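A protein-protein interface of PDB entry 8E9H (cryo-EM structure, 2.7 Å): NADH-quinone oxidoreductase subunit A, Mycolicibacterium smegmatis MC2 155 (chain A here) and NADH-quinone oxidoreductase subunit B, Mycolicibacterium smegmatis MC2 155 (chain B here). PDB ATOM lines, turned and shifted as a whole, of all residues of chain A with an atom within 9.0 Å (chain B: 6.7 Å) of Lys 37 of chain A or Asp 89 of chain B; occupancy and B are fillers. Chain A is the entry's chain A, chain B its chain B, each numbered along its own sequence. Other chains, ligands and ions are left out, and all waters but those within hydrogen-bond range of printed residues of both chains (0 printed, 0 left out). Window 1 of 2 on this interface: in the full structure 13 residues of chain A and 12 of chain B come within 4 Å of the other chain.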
ATOM      1  N   PRO A  30      -2.077  -1.857 -30.714  1.00  0.00           N
ATOM      2  CA  PRO A  30      -1.703  -3.269 -30.615  1.00  0.00           C
ATOM      3  C   PRO A  30      -2.921  -4.175 -30.650  1.00  0.00           C
ATOM      4  O   PRO A  30      -4.018  -3.812 -30.228  1.00  0.00           O
ATOM      5  CB  PRO A  30      -0.991  -3.362 -29.260  1.00  0.00           C
ATOM      6  CG  PRO A  30      -0.815  -1.950 -28.789  1.00  0.00           C
ATOM      7  CD  PRO A  30      -1.888  -1.159 -29.435  1.00  0.00           C
ATOM      8  N   ARG A  31      -2.707  -5.376 -31.174  1.00  0.00           N
ATOM      9  CA  ARG A  31      -3.708  -6.428 -31.141  1.00  0.00           C
ATOM     10  C   ARG A  31      -3.084  -7.669 -30.529  1.00  0.00           C
ATOM     11  O   ARG A  31      -1.995  -8.087 -30.926  1.00  0.00           O
ATOM     12  CB  ARG A  31      -4.248  -6.745 -32.535  1.00  0.00           C
ATOM     13  CG  ARG A  31      -4.748  -5.531 -33.284  1.00  0.00           C
ATOM     14  CD  ARG A  31      -5.753  -5.923 -34.343  1.00  0.00           C
ATOM     15  NE  ARG A  31      -7.102  -5.972 -33.790  1.00  0.00           N
ATOM     16  CZ  ARG A  31      -7.895  -7.035 -33.801  1.00  0.00           C
ATOM     17  NH1 ARG A  31      -7.515  -8.182 -34.343  1.00  0.00           N
ATOM     18  NH2 ARG A  31      -9.101  -6.947 -33.251  1.00  0.00           N
ATOM     19  N   ARG A  32      -3.782  -8.253 -29.559  1.00  0.00           N
ATOM     20  CA  ARG A  32      -3.253  -9.399 -28.828  1.00  0.00           C
ATOM     21  C   ARG A  32      -4.427 -10.327 -28.536  1.00  0.00           C
ATOM     22  O   ARG A  32      -5.268 -10.016 -27.688  1.00  0.00           O
ATOM     23  CB  ARG A  32      -2.559  -8.956 -27.549  1.00  0.00           C
ATOM     24  CG  ARG A  32      -2.005 -10.090 -26.711  1.00  0.00           C
ATOM     25  CD  ARG A  32      -0.803 -10.724 -27.375  1.00  0.00           C
ATOM     26  NE  ARG A  32      -0.383 -11.940 -26.692  1.00  0.00           N
ATOM     27  CZ  ARG A  32       0.669 -12.667 -27.037  1.00  0.00           C
ATOM     28  NH1 ARG A  32       1.440 -12.326 -28.057  1.00  0.00           N
ATOM     29  NH2 ARG A  32       0.952 -13.767 -26.347  1.00  0.00           N
ATOM     30  N   PHE A  33      -4.483 -11.451 -29.242  1.00  0.00           N
ATOM     31  CA  PHE A  33      -5.557 -12.402 -29.007  1.00  0.00           C
ATOM     32  C   PHE A  33      -5.505 -12.906 -27.575  1.00  0.00           C
ATOM     33  O   PHE A  33      -4.439 -13.264 -27.067  1.00  0.00           O
ATOM     34  CB  PHE A  33      -5.461 -13.573 -29.977  1.00  0.00           C
ATOM     35  CG  PHE A  33      -6.441 -14.665 -29.685  1.00  0.00           C
ATOM     36  CD1 PHE A  33      -6.084 -15.742 -28.898  1.00  0.00           C
ATOM     37  CD2 PHE A  33      -7.731 -14.601 -30.174  1.00  0.00           C
ATOM     38  CE1 PHE A  33      -6.989 -16.742 -28.619  1.00  0.00           C
ATOM     39  CE2 PHE A  33      -8.639 -15.598 -29.898  1.00  0.00           C
ATOM     40  CZ  PHE A  33      -8.267 -16.669 -29.120  1.00  0.00           C
ATOM     41  N   ASN A  34      -6.662 -12.936 -26.926  1.00  0.00           N
ATOM     42  CA  ASN A  34      -6.761 -13.424 -25.555  1.00  0.00           C
ATOM     43  C   ASN A  34      -8.196 -13.857 -25.323  1.00  0.00           C
ATOM     44  O   ASN A  34      -9.110 -13.035 -25.424  1.00  0.00           O
ATOM     45  CB  ASN A  34      -6.347 -12.345 -24.561  1.00  0.00           C
ATOM     46  CG  ASN A  34      -6.524 -12.779 -23.124  1.00  0.00           C
ATOM     47  OD1 ASN A  34      -7.591 -13.241 -22.729  1.00  0.00           O
ATOM     48  ND2 ASN A  34      -5.473 -12.629 -22.330  1.00  0.00           N
ATOM     49  N   ARG A  35      -8.395 -15.132 -25.001  1.00  0.00           N
ATOM     50  CA  ARG A  35      -9.750 -15.648 -24.855  1.00  0.00           C
ATOM     51  C   ARG A  35     -10.512 -14.879 -23.786  1.00  0.00           C
ATOM     52  O   ARG A  35     -11.687 -14.544 -23.968  1.00  0.00           O
ATOM     53  CB  ARG A  35      -9.703 -17.135 -24.520  1.00  0.00           C
ATOM     54  CG  ARG A  35      -9.223 -17.982 -25.671  1.00  0.00           C
ATOM     55  CD  ARG A  35      -9.127 -19.440 -25.293  1.00  0.00           C
ATOM     56  NE  ARG A  35      -8.820 -20.260 -26.456  1.00  0.00           N
ATOM     57  CZ  ARG A  35      -7.624 -20.333 -27.023  1.00  0.00           C
ATOM     58  NH1 ARG A  35      -6.591 -19.655 -26.549  1.00  0.00           N
ATOM     59  NH2 ARG A  35      -7.460 -21.105 -28.094  1.00  0.00           N
ATOM     60  N   SER A  36      -9.860 -14.590 -22.661  1.00  0.00           N
ATOM     61  CA  SER A  36     -10.518 -13.817 -21.616  1.00  0.00           C
ATOM     62  C   SER A  36     -10.858 -12.415 -22.093  1.00  0.00           C
ATOM     63  O   SER A  36     -11.908 -11.876 -21.730  1.00  0.00           O
ATOM     64  CB  SER A  36      -9.634 -13.753 -20.375  1.00  0.00           C
ATOM     65  OG  SER A  36      -9.327 -15.053 -19.908  1.00  0.00           O
ATOM     66  N   LYS A  37      -9.990 -11.807 -22.899  1.00  0.00           N
ATOM     67  CA  LYS A  37     -10.282 -10.477 -23.418  1.00  0.00           C
ATOM     68  C   LYS A  37     -11.518 -10.497 -24.305  1.00  0.00           C
ATOM     69  O   LYS A  37     -12.369  -9.605 -24.219  1.00  0.00           O
ATOM     70  CB  LYS A  37      -9.078  -9.945 -24.195  1.00  0.00           C
ATOM     71  CG  LYS A  37      -9.245  -8.524 -24.694  1.00  0.00           C
ATOM     72  CD  LYS A  37      -8.110  -8.116 -25.610  1.00  0.00           C
ATOM     73  CE  LYS A  37      -6.819  -7.917 -24.844  1.00  0.00           C
ATOM     74  NZ  LYS A  37      -5.659  -7.744 -25.755  1.00  0.00           N
ATOM     75  N   LEU A  38     -11.637 -11.509 -25.162  1.00  0.00           N
ATOM     76  CA  LEU A  38     -12.694 -11.507 -26.163  1.00  0.00           C
ATOM     77  C   LEU A  38     -14.052 -11.876 -25.585  1.00  0.00           C
ATOM     78  O   LEU A  38     -15.079 -11.445 -26.118  1.00  0.00           O
ATOM     79  CB  LEU A  38     -12.335 -12.464 -27.296  1.00  0.00           C
ATOM     80  CG  LEU A  38     -11.006 -12.179 -27.994  1.00  0.00           C
ATOM     81  CD1 LEU A  38     -10.867 -13.054 -29.221  1.00  0.00           C
ATOM     82  CD2 LEU A  38     -10.884 -10.715 -28.363  1.00  0.00           C
ATOM     83  N   GLU A  39     -14.093 -12.665 -24.519  1.00  0.00           N
ATOM     84  CA  GLU A  39     -15.377 -13.106 -24.002  1.00  0.00           C
ATOM     85  C   GLU A  39     -16.117 -11.944 -23.346  1.00  0.00           C
ATOM     86  O   GLU A  39     -15.539 -10.908 -23.012  1.00  0.00           O
ATOM     87  CB  GLU A  39     -15.197 -14.254 -23.014  1.00  0.00           C
ATOM     88  CG  GLU A  39     -14.521 -13.873 -21.721  1.00  0.00           C
ATOM     89  CD  GLU A  39     -14.126 -15.086 -20.906  1.00  0.00           C
ATOM     90  OE1 GLU A  39     -14.226 -16.213 -21.431  1.00  0.00           O
ATOM     91  OE2 GLU A  39     -13.715 -14.915 -19.740  1.00  0.00           O
ATOM     92  N   ALA A  40     -17.421 -12.133 -23.170  1.00  0.00           N
ATOM     93  CA  ALA A  40     -18.286 -11.054 -22.723  1.00  0.00           C
ATOM     94  C   ALA A  40     -17.824 -10.505 -21.381  1.00  0.00           C
ATOM     95  O   ALA A  40     -17.169 -11.185 -20.590  1.00  0.00           O
ATOM     96  CB  ALA A  40     -19.729 -11.543 -22.610  1.00  0.00           C
ATOM     97  N   TYR A  41     -18.182  -9.250 -21.128  1.00  0.00           N
ATOM     98  CA  TYR A  41     -17.896  -8.593 -19.862  1.00  0.00           C
ATOM     99  C   TYR A  41     -19.049  -8.864 -18.909  1.00  0.00           C
ATOM    100  O   TYR A  41     -20.203  -8.556 -19.222  1.00  0.00           O
ATOM    101  CB  TYR A  41     -17.710  -7.090 -20.044  1.00  0.00           C
ATOM    102  CG  TYR A  41     -17.782  -6.331 -18.747  1.00  0.00           C
ATOM    103  CD1 TYR A  41     -16.710  -6.313 -17.873  1.00  0.00           C
ATOM    104  CD2 TYR A  41     -18.930  -5.648 -18.388  1.00  0.00           C
ATOM    105  CE1 TYR A  41     -16.774  -5.628 -16.689  1.00  0.00           C
ATOM    106  CE2 TYR A  41     -19.002  -4.963 -17.204  1.00  0.00           C
ATOM    107  CZ  TYR A  41     -17.921  -4.953 -16.358  1.00  0.00           C
ATOM    108  OH  TYR A  41     -17.987  -4.268 -15.171  1.00  0.00           O
ATOM    109  N   GLY A  44     -16.342  -9.036 -14.333  1.00  0.00           N
ATOM    110  CA  GLY A  44     -15.184  -9.779 -13.883  1.00  0.00           C
ATOM    111  C   GLY A  44     -15.449 -11.254 -13.677  1.00  0.00           C
ATOM    112  O   GLY A  44     -14.521 -12.065 -13.706  1.00  0.00           O
ATOM    113  N   PRO A  47     -18.082 -15.539 -17.810  1.00  0.00           N
ATOM    114  CA  PRO A  47     -19.375 -15.493 -18.495  1.00  0.00           C
ATOM    115  C   PRO A  47     -20.094 -16.826 -18.387  1.00  0.00           C
ATOM    116  O   PRO A  47     -19.471 -17.888 -18.377  1.00  0.00           O
ATOM    117  CB  PRO A  47     -18.996 -15.167 -19.943  1.00  0.00           C
ATOM    118  CG  PRO A  47     -17.611 -15.665 -20.078  1.00  0.00           C
ATOM    119  CD  PRO A  47     -16.965 -15.402 -18.756  1.00  0.00           C
ATOM    120  N   PRO B  64     -13.953  -2.314 -18.340  1.00  0.00           N
ATOM    121  CA  PRO B  64     -12.518  -2.486 -18.587  1.00  0.00           C
ATOM    122  C   PRO B  64     -12.119  -2.163 -20.012  1.00  0.00           C
ATOM    123  O   PRO B  64     -10.941  -1.883 -20.262  1.00  0.00           O
ATOM    124  CB  PRO B  64     -12.281  -3.963 -18.251  1.00  0.00           C
ATOM    125  CG  PRO B  64     -13.598  -4.605 -18.403  1.00  0.00           C
ATOM    126  CD  PRO B  64     -14.612  -3.587 -18.017  1.00  0.00           C
ATOM    127  N   ARG B  65     -13.060  -2.183 -20.956  1.00  0.00           N
ATOM    128  CA  ARG B  65     -12.700  -1.956 -22.350  1.00  0.00           C
ATOM    129  C   ARG B  65     -12.094  -0.575 -22.545  1.00  0.00           C
ATOM    130  O   ARG B  65     -11.084  -0.428 -23.240  1.00  0.00           O
ATOM    131  CB  ARG B  65     -13.923  -2.121 -23.246  1.00  0.00           C
ATOM    132  CG  ARG B  65     -14.725  -3.382 -23.003  1.00  0.00           C
ATOM    133  CD  ARG B  65     -13.853  -4.607 -22.859  1.00  0.00           C
ATOM    134  NE  ARG B  65     -14.632  -5.828 -23.024  1.00  0.00           N
ATOM    135  CZ  ARG B  65     -14.121  -7.010 -23.335  1.00  0.00           C
ATOM    136  NH1 ARG B  65     -12.822  -7.180 -23.505  1.00  0.00           N
ATOM    137  NH2 ARG B  65     -14.936  -8.050 -23.482  1.00  0.00           N
ATOM    138  N   MET B  70      -5.198   0.101 -14.689  1.00  0.00           N
ATOM    139  CA  MET B  70      -5.904  -0.594 -13.620  1.00  0.00           C
ATOM    140  C   MET B  70      -5.191  -0.291 -12.313  1.00  0.00           C
ATOM    141  O   MET B  70      -4.225  -0.961 -11.948  1.00  0.00           O
ATOM    142  CB  MET B  70      -5.965  -2.092 -13.878  1.00  0.00           C
ATOM    143  CG  MET B  70      -6.615  -2.868 -12.743  1.00  0.00           C
ATOM    144  SD  MET B  70      -6.111  -4.586 -12.672  1.00  0.00           S
ATOM    145  CE  MET B  70      -7.470  -5.330 -13.556  1.00  0.00           C
ATOM    146  N   LEU B  84      -9.926 -10.106 -10.561  1.00  0.00           N
ATOM    147  CA  LEU B  84      -8.992  -9.056 -10.943  1.00  0.00           C
ATOM    148  C   LEU B  84      -8.288  -9.406 -12.244  1.00  0.00           C
ATOM    149  O   LEU B  84      -8.114  -8.549 -13.115  1.00  0.00           O
ATOM    150  CB  LEU B  84      -7.982  -8.835  -9.822  1.00  0.00           C
ATOM    151  CG  LEU B  84      -7.085  -7.610  -9.961  1.00  0.00           C
ATOM    152  CD1 LEU B  84      -6.779  -7.046  -8.593  1.00  0.00           C
ATOM    153  CD2 LEU B  84      -5.802  -7.955 -10.689  1.00  0.00           C
ATOM    154  N   ARG B  85      -7.874 -10.664 -12.396  1.00  0.00           N
ATOM    155  CA  ARG B  85      -7.238 -11.073 -13.641  1.00  0.00           C
ATOM    156  C   ARG B  85      -8.211 -10.979 -14.804  1.00  0.00           C
ATOM    157  O   ARG B  85      -7.826 -10.594 -15.911  1.00  0.00           O
ATOM    158  CB  ARG B  85      -6.693 -12.492 -13.523  1.00  0.00           C
ATOM    159  CG  ARG B  85      -6.039 -13.006 -14.798  1.00  0.00           C
ATOM    160  CD  ARG B  85      -4.680 -12.389 -15.012  1.00  0.00           C
ATOM    161  NE  ARG B  85      -4.372 -12.237 -16.427  1.00  0.00           N
ATOM    162  CZ  ARG B  85      -3.160 -12.005 -16.909  1.00  0.00           C
ATOM    163  NH1 ARG B  85      -2.110 -11.893 -16.114  1.00  0.00           N
ATOM    164  NH2 ARG B  85      -2.996 -11.881 -18.221  1.00  0.00           N
ATOM    165  N   GLN B  86      -9.472 -11.348 -14.583  1.00  0.00           N
ATOM    166  CA  GLN B  86     -10.459 -11.227 -15.648  1.00  0.00           C
ATOM    167  C   GLN B  86     -10.616  -9.778 -16.075  1.00  0.00           C
ATOM    168  O   GLN B  86     -10.680  -9.477 -17.271  1.00  0.00           O
ATOM    169  CB  GLN B  86     -11.798 -11.797 -15.193  1.00  0.00           C
ATOM    170  CG  GLN B  86     -12.845 -11.832 -16.283  1.00  0.00           C
ATOM    171  CD  GLN B  86     -12.529 -12.845 -17.351  1.00  0.00           C
ATOM    172  OE1 GLN B  86     -11.545 -13.575 -17.258  1.00  0.00           O
ATOM    173  NE2 GLN B  86     -13.361 -12.895 -18.379  1.00  0.00           N
ATOM    174  N   ILE B  87     -10.678  -8.864 -15.109  1.00  0.00           N
ATOM    175  CA  ILE B  87     -10.801  -7.450 -15.442  1.00  0.00           C
ATOM    176  C   ILE B  87      -9.579  -6.990 -16.222  1.00  0.00           C
ATOM    177  O   ILE B  87      -9.694  -6.292 -17.234  1.00  0.00           O
ATOM    178  CB  ILE B  87     -11.003  -6.614 -14.169  1.00  0.00           C
ATOM    179  CG1 ILE B  87     -12.337  -6.960 -13.508  1.00  0.00           C
ATOM    180  CG2 ILE B  87     -10.943  -5.138 -14.494  1.00  0.00           C
ATOM    181  CD1 ILE B  87     -13.543  -6.752 -14.394  1.00  0.00           C
ATOM    182  N   TYR B  88      -8.390  -7.383 -15.769  1.00  0.00           N
ATOM    183  CA  TYR B  88      -7.177  -6.977 -16.466  1.00  0.00           C
ATOM    184  C   TYR B  88      -7.174  -7.487 -17.898  1.00  0.00           C
ATOM    185  O   TYR B  88      -6.840  -6.748 -18.829  1.00  0.00           O
ATOM    186  CB  TYR B  88      -5.944  -7.486 -15.727  1.00  0.00           C
ATOM    187  CG  TYR B  88      -4.663  -7.256 -16.485  1.00  0.00           C
ATOM    188  CD1 TYR B  88      -4.042  -6.021 -16.470  1.00  0.00           C
ATOM    189  CD2 TYR B  88      -4.077  -8.273 -17.217  1.00  0.00           C
ATOM    190  CE1 TYR B  88      -2.875  -5.805 -17.157  1.00  0.00           C
ATOM    191  CE2 TYR B  88      -2.909  -8.066 -17.908  1.00  0.00           C
ATOM    192  CZ  TYR B  88      -2.312  -6.830 -17.876  1.00  0.00           C
ATOM    193  OH  TYR B  88      -1.145  -6.618 -18.566  1.00  0.00           O
ATOM    194  N   ASP B  89      -7.548  -8.750 -18.095  1.00  0.00           N
ATOM    195  CA  ASP B  89      -7.594  -9.297 -19.443  1.00  0.00           C
ATOM    196  C   ASP B  89      -8.611  -8.569 -20.301  1.00  0.00           C
ATOM    197  O   ASP B  89      -8.349  -8.294 -21.476  1.00  0.00           O
ATOM    198  CB  ASP B  89      -7.919 -10.786 -19.394  1.00  0.00           C
ATOM    199  CG  ASP B  89      -6.712 -11.631 -19.066  1.00  0.00           C
ATOM    200  OD1 ASP B  89      -5.628 -11.359 -19.621  1.00  0.00           O
ATOM    201  OD2 ASP B  89      -6.845 -12.572 -18.258  1.00  0.00           O
ATOM    202  N   GLN B  90      -9.772  -8.248 -19.740  1.00  0.00           N
ATOM    203  CA  GLN B  90     -10.822  -7.604 -20.512  1.00  0.00           C
ATOM    204  C   GLN B  90     -10.512  -6.151 -20.833  1.00  0.00           C
ATOM    205  O   GLN B  90     -11.223  -5.553 -21.644  1.00  0.00           O
ATOM    206  CB  GLN B  90     -12.148  -7.719 -19.769  1.00  0.00           C
ATOM    207  CG  GLN B  90     -12.709  -9.122 -19.824  1.00  0.00           C
ATOM    208  CD  GLN B  90     -14.086  -9.225 -19.235  1.00  0.00           C
ATOM    209  OE1 GLN B  90     -14.497  -8.386 -18.441  1.00  0.00           O
ATOM    210  NE2 GLN B  90     -14.810 -10.268 -19.613  1.00  0.00           N
ATOM    211  N   MET B  91      -9.486  -5.568 -20.222  1.00  0.00           N
ATOM    212  CA  MET B  91      -8.925  -4.342 -20.758  1.00  0.00           C
ATOM    213  C   MET B  91      -8.130  -4.668 -22.017  1.00  0.00           C
ATOM    214  O   MET B  91      -7.704  -5.804 -22.232  1.00  0.00           O
ATOM    215  CB  MET B  91      -8.031  -3.653 -19.731  1.00  0.00           C
ATOM    216  CG  MET B  91      -8.551  -3.705 -18.313  1.00  0.00           C
ATOM    217  SD  MET B  91      -7.976  -2.332 -17.304  1.00  0.00           S
ATOM    218  CE  MET B  91      -6.217  -2.418 -17.595  1.00  0.00           C
ATOM    219  N   VAL B  92      -7.925  -3.659 -22.855  1.00  0.00           N
ATOM    220  CA  VAL B  92      -7.314  -3.864 -24.159  1.00  0.00           C
ATOM    221  C   VAL B  92      -6.016  -3.075 -24.240  1.00  0.00           C
ATOM    222  O   VAL B  92      -5.851  -2.045 -23.581  1.00  0.00           O
ATOM    223  CB  VAL B  92      -8.273  -3.468 -25.299  1.00  0.00           C
ATOM    224  CG1 VAL B  92      -9.548  -4.275 -25.211  1.00  0.00           C
ATOM    225  CG2 VAL B  92      -8.579  -1.995 -25.254  1.00  0.00           C
ATOM    226  N   GLU B  93      -5.095  -3.564 -25.068  1.00  0.00           N
ATOM    227  CA  GLU B  93      -3.757  -2.999 -25.115  1.00  0.00           C
ATOM    228  C   GLU B  93      -3.812  -1.541 -25.566  1.00  0.00           C
ATOM    229  O   GLU B  93      -4.685  -1.157 -26.347  1.00  0.00           O
ATOM    230  CB  GLU B  93      -2.869  -3.780 -26.080  1.00  0.00           C
ATOM    231  CG  GLU B  93      -2.918  -5.282 -25.938  1.00  0.00           C
ATOM    232  CD  GLU B  93      -2.888  -5.735 -24.502  1.00  0.00           C
ATOM    233  OE1 GLU B  93      -2.096  -5.174 -23.718  1.00  0.00           O
ATOM    234  OE2 GLU B  93      -3.648  -6.665 -24.161  1.00  0.00           O
ATOM    235  N   LYS B  95      -1.992  -1.733 -21.732  1.00  0.00           N
ATOM    236  CA  LYS B  95      -2.525  -1.822 -20.383  1.00  0.00           C
ATOM    237  C   LYS B  95      -1.413  -1.555 -19.384  1.00  0.00           C
ATOM    238  O   LYS B  95      -0.260  -1.934 -19.601  1.00  0.00           O
ATOM    239  CB  LYS B  95      -3.127  -3.199 -20.102  1.00  0.00           C
ATOM    240  CG  LYS B  95      -4.283  -3.563 -20.997  1.00  0.00           C
ATOM    241  CD  LYS B  95      -4.850  -4.922 -20.641  1.00  0.00           C
ATOM    242  CE  LYS B  95      -3.920  -6.043 -21.026  1.00  0.00           C
ATOM    243  NZ  LYS B  95      -4.605  -7.361 -20.972  1.00  0.00           N
ATOM    244  N   VAL B 123      -1.218 -10.270 -12.163  1.00  0.00           N
ATOM    245  CA  VAL B 123      -1.144  -9.380 -13.323  1.00  0.00           C
ATOM    246  C   VAL B 123       0.153  -8.600 -13.271  1.00  0.00           C
ATOM    247  O   VAL B 123       0.651  -8.249 -12.195  1.00  0.00           O
ATOM    248  CB  VAL B 123      -2.330  -8.399 -13.371  1.00  0.00           C
ATOM    249  CG1 VAL B 123      -3.619  -9.143 -13.622  1.00  0.00           C
ATOM    250  CG2 VAL B 123      -2.424  -7.622 -12.084  1.00  0.00           C
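Hydrophobic or aromatic side chains of chain A that line the printed part of chain B: Pro 30 and Tyr 41.
Of the 15 printed residues of chain B, 8 touch a printed residue of chain A.
Printed residues of chain B that touch a printed residue of chain A: Pro 64, Arg 65, Gln 86, Ile 87, Asp 89, Gln 90, Met 91 and Glu 93.
Among the printed residues, 17 pairs touch across the chains.
NH1 of Arg 65 of chain B lies within hydrogen-bond range of O of Gln 90 of chain B (2.9 Å).
The side-chain amide nitrogen (NE2) of Gln 90 of chain B lies close to the side-chain amide nitrogen (NE2) of Gln 86 of chain B, 3.2 Å away.
NZ of Lys 95 of chain B lies within salt-bridge range of OE2 of Glu 93 of chain B, 3.4 Å away.
The backbone carbonyl oxygen of Arg 32 of chain A lies within hydrogen-bond range of the side-chain amino group of Lys 37 of chain A (3.0 Å).
OD1 of Asn 34 of chain A lies within hydrogen-bond range of N of Ser 36 of chain A (2.6 Å).
The backbone NH (N) of Lys 37 of chain A is in hydrogen-bond range of the side-chain amide oxygen (OD1) of Asn 34 of chain A, at 2.8 Å.
The backbone carbonyl oxygen of Lys 37 of chain A is in hydrogen-bond range of the guanidinium group of Arg 65 of chain B.
The guanidinium group of Arg 65 of chain B is in hydrogen-bond range of the backbone carbonyl oxygen of Glu 39 of chain A, at 3.0 Å.
NE2 of Gln 86 of chain B is in hydrogen-bond range of OE2 of Glu 39 of chain A (2.5 Å).
The side-chain amide nitrogen of Asn 34 of chain A is in hydrogen-bond range of the side-chain carboxylate of Asp 89 of chain B, 3.0 Å away.
The backbone carbonyl oxygen (O) of Ala 40 of chain A lies within hydrogen-bond range of the side-chain amide nitrogen (NE2) of Gln 90 of chain B (2.7 Å).
The side-chain carboxylate (OE2) of Glu 93 of chain B is in salt-bridge range of the side-chain amino group (NZ) of Lys 37 of chain A, 2.8 Å away.
Lys 37 of chain A touches just these residues of chain B: Arg 65, Asp 89, Met 91 and Glu 93.
Of chain A, only Asn 34 (3.0 Å), Ser 36 (3.6 Å) and Lys 37 (3.3 Å) come within 4 Å of Asp 89 of chain B.
Of the printed residues of chain B, Gly 44 of chain A touches Gln 86 (3.1 Å) and Ile 87 (3.5 Å).
Of the printed residues of chain A, Glu 93 of chain B touches Pro 30 and Lys 37.
Printed residues of chain A within 4 Å of Pro 64 of chain B: Tyr 41 (3.3 Å).
Printed residues of chain A within 4 Å of Arg 65 of chain B: Lys 37 (2.6 Å) and Glu 39 (3.0 Å).
Printed residues of chain B within 4 Å of Tyr 41 of chain A: Pro 64 and Gln 90.
The nearest printed residue of chain B that does not touch Lys 37 of chain A is Val 92 of chain B (4.1 Å).
The nearest residue of chain A that does not touch Asp 89 of chain B is Leu 38 of chain A (5.9 Å).
The nearest printed residue of chain A that does not touch Glu 93 of chain B is Arg 32 of chain A (4.03 Å).
CB of Pro 30 of chain A touches CB of Glu 93 of chain B (3.7 Å).
Gln 86 of chain B touches Ser 36 of chain A.
Ser 36 of chain A touches Asp 89 of chain B.
Lys 37 of chain A touches Asp 89 of chain B (CB to O, 3.3 Å).
O of Met 91 of chain B touches CE of Lys 37 of chain A, at 3.5 Å.
O of Glu 39 of chain A touches NE2 of Gln 90 of chain B, 3.5 Å away.
Pro 64 of chain B touches Tyr 41 of chain A.
Tyr 41 of chain A touches Gln 90 of chain B (CD1 to OE1, 3.1 Å).
O of Gly 44 of chain A touches CG of Gln 86 of chain B, at 3.1 Å.
Gly 44 of chain A touches Ile 87 of chain B.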
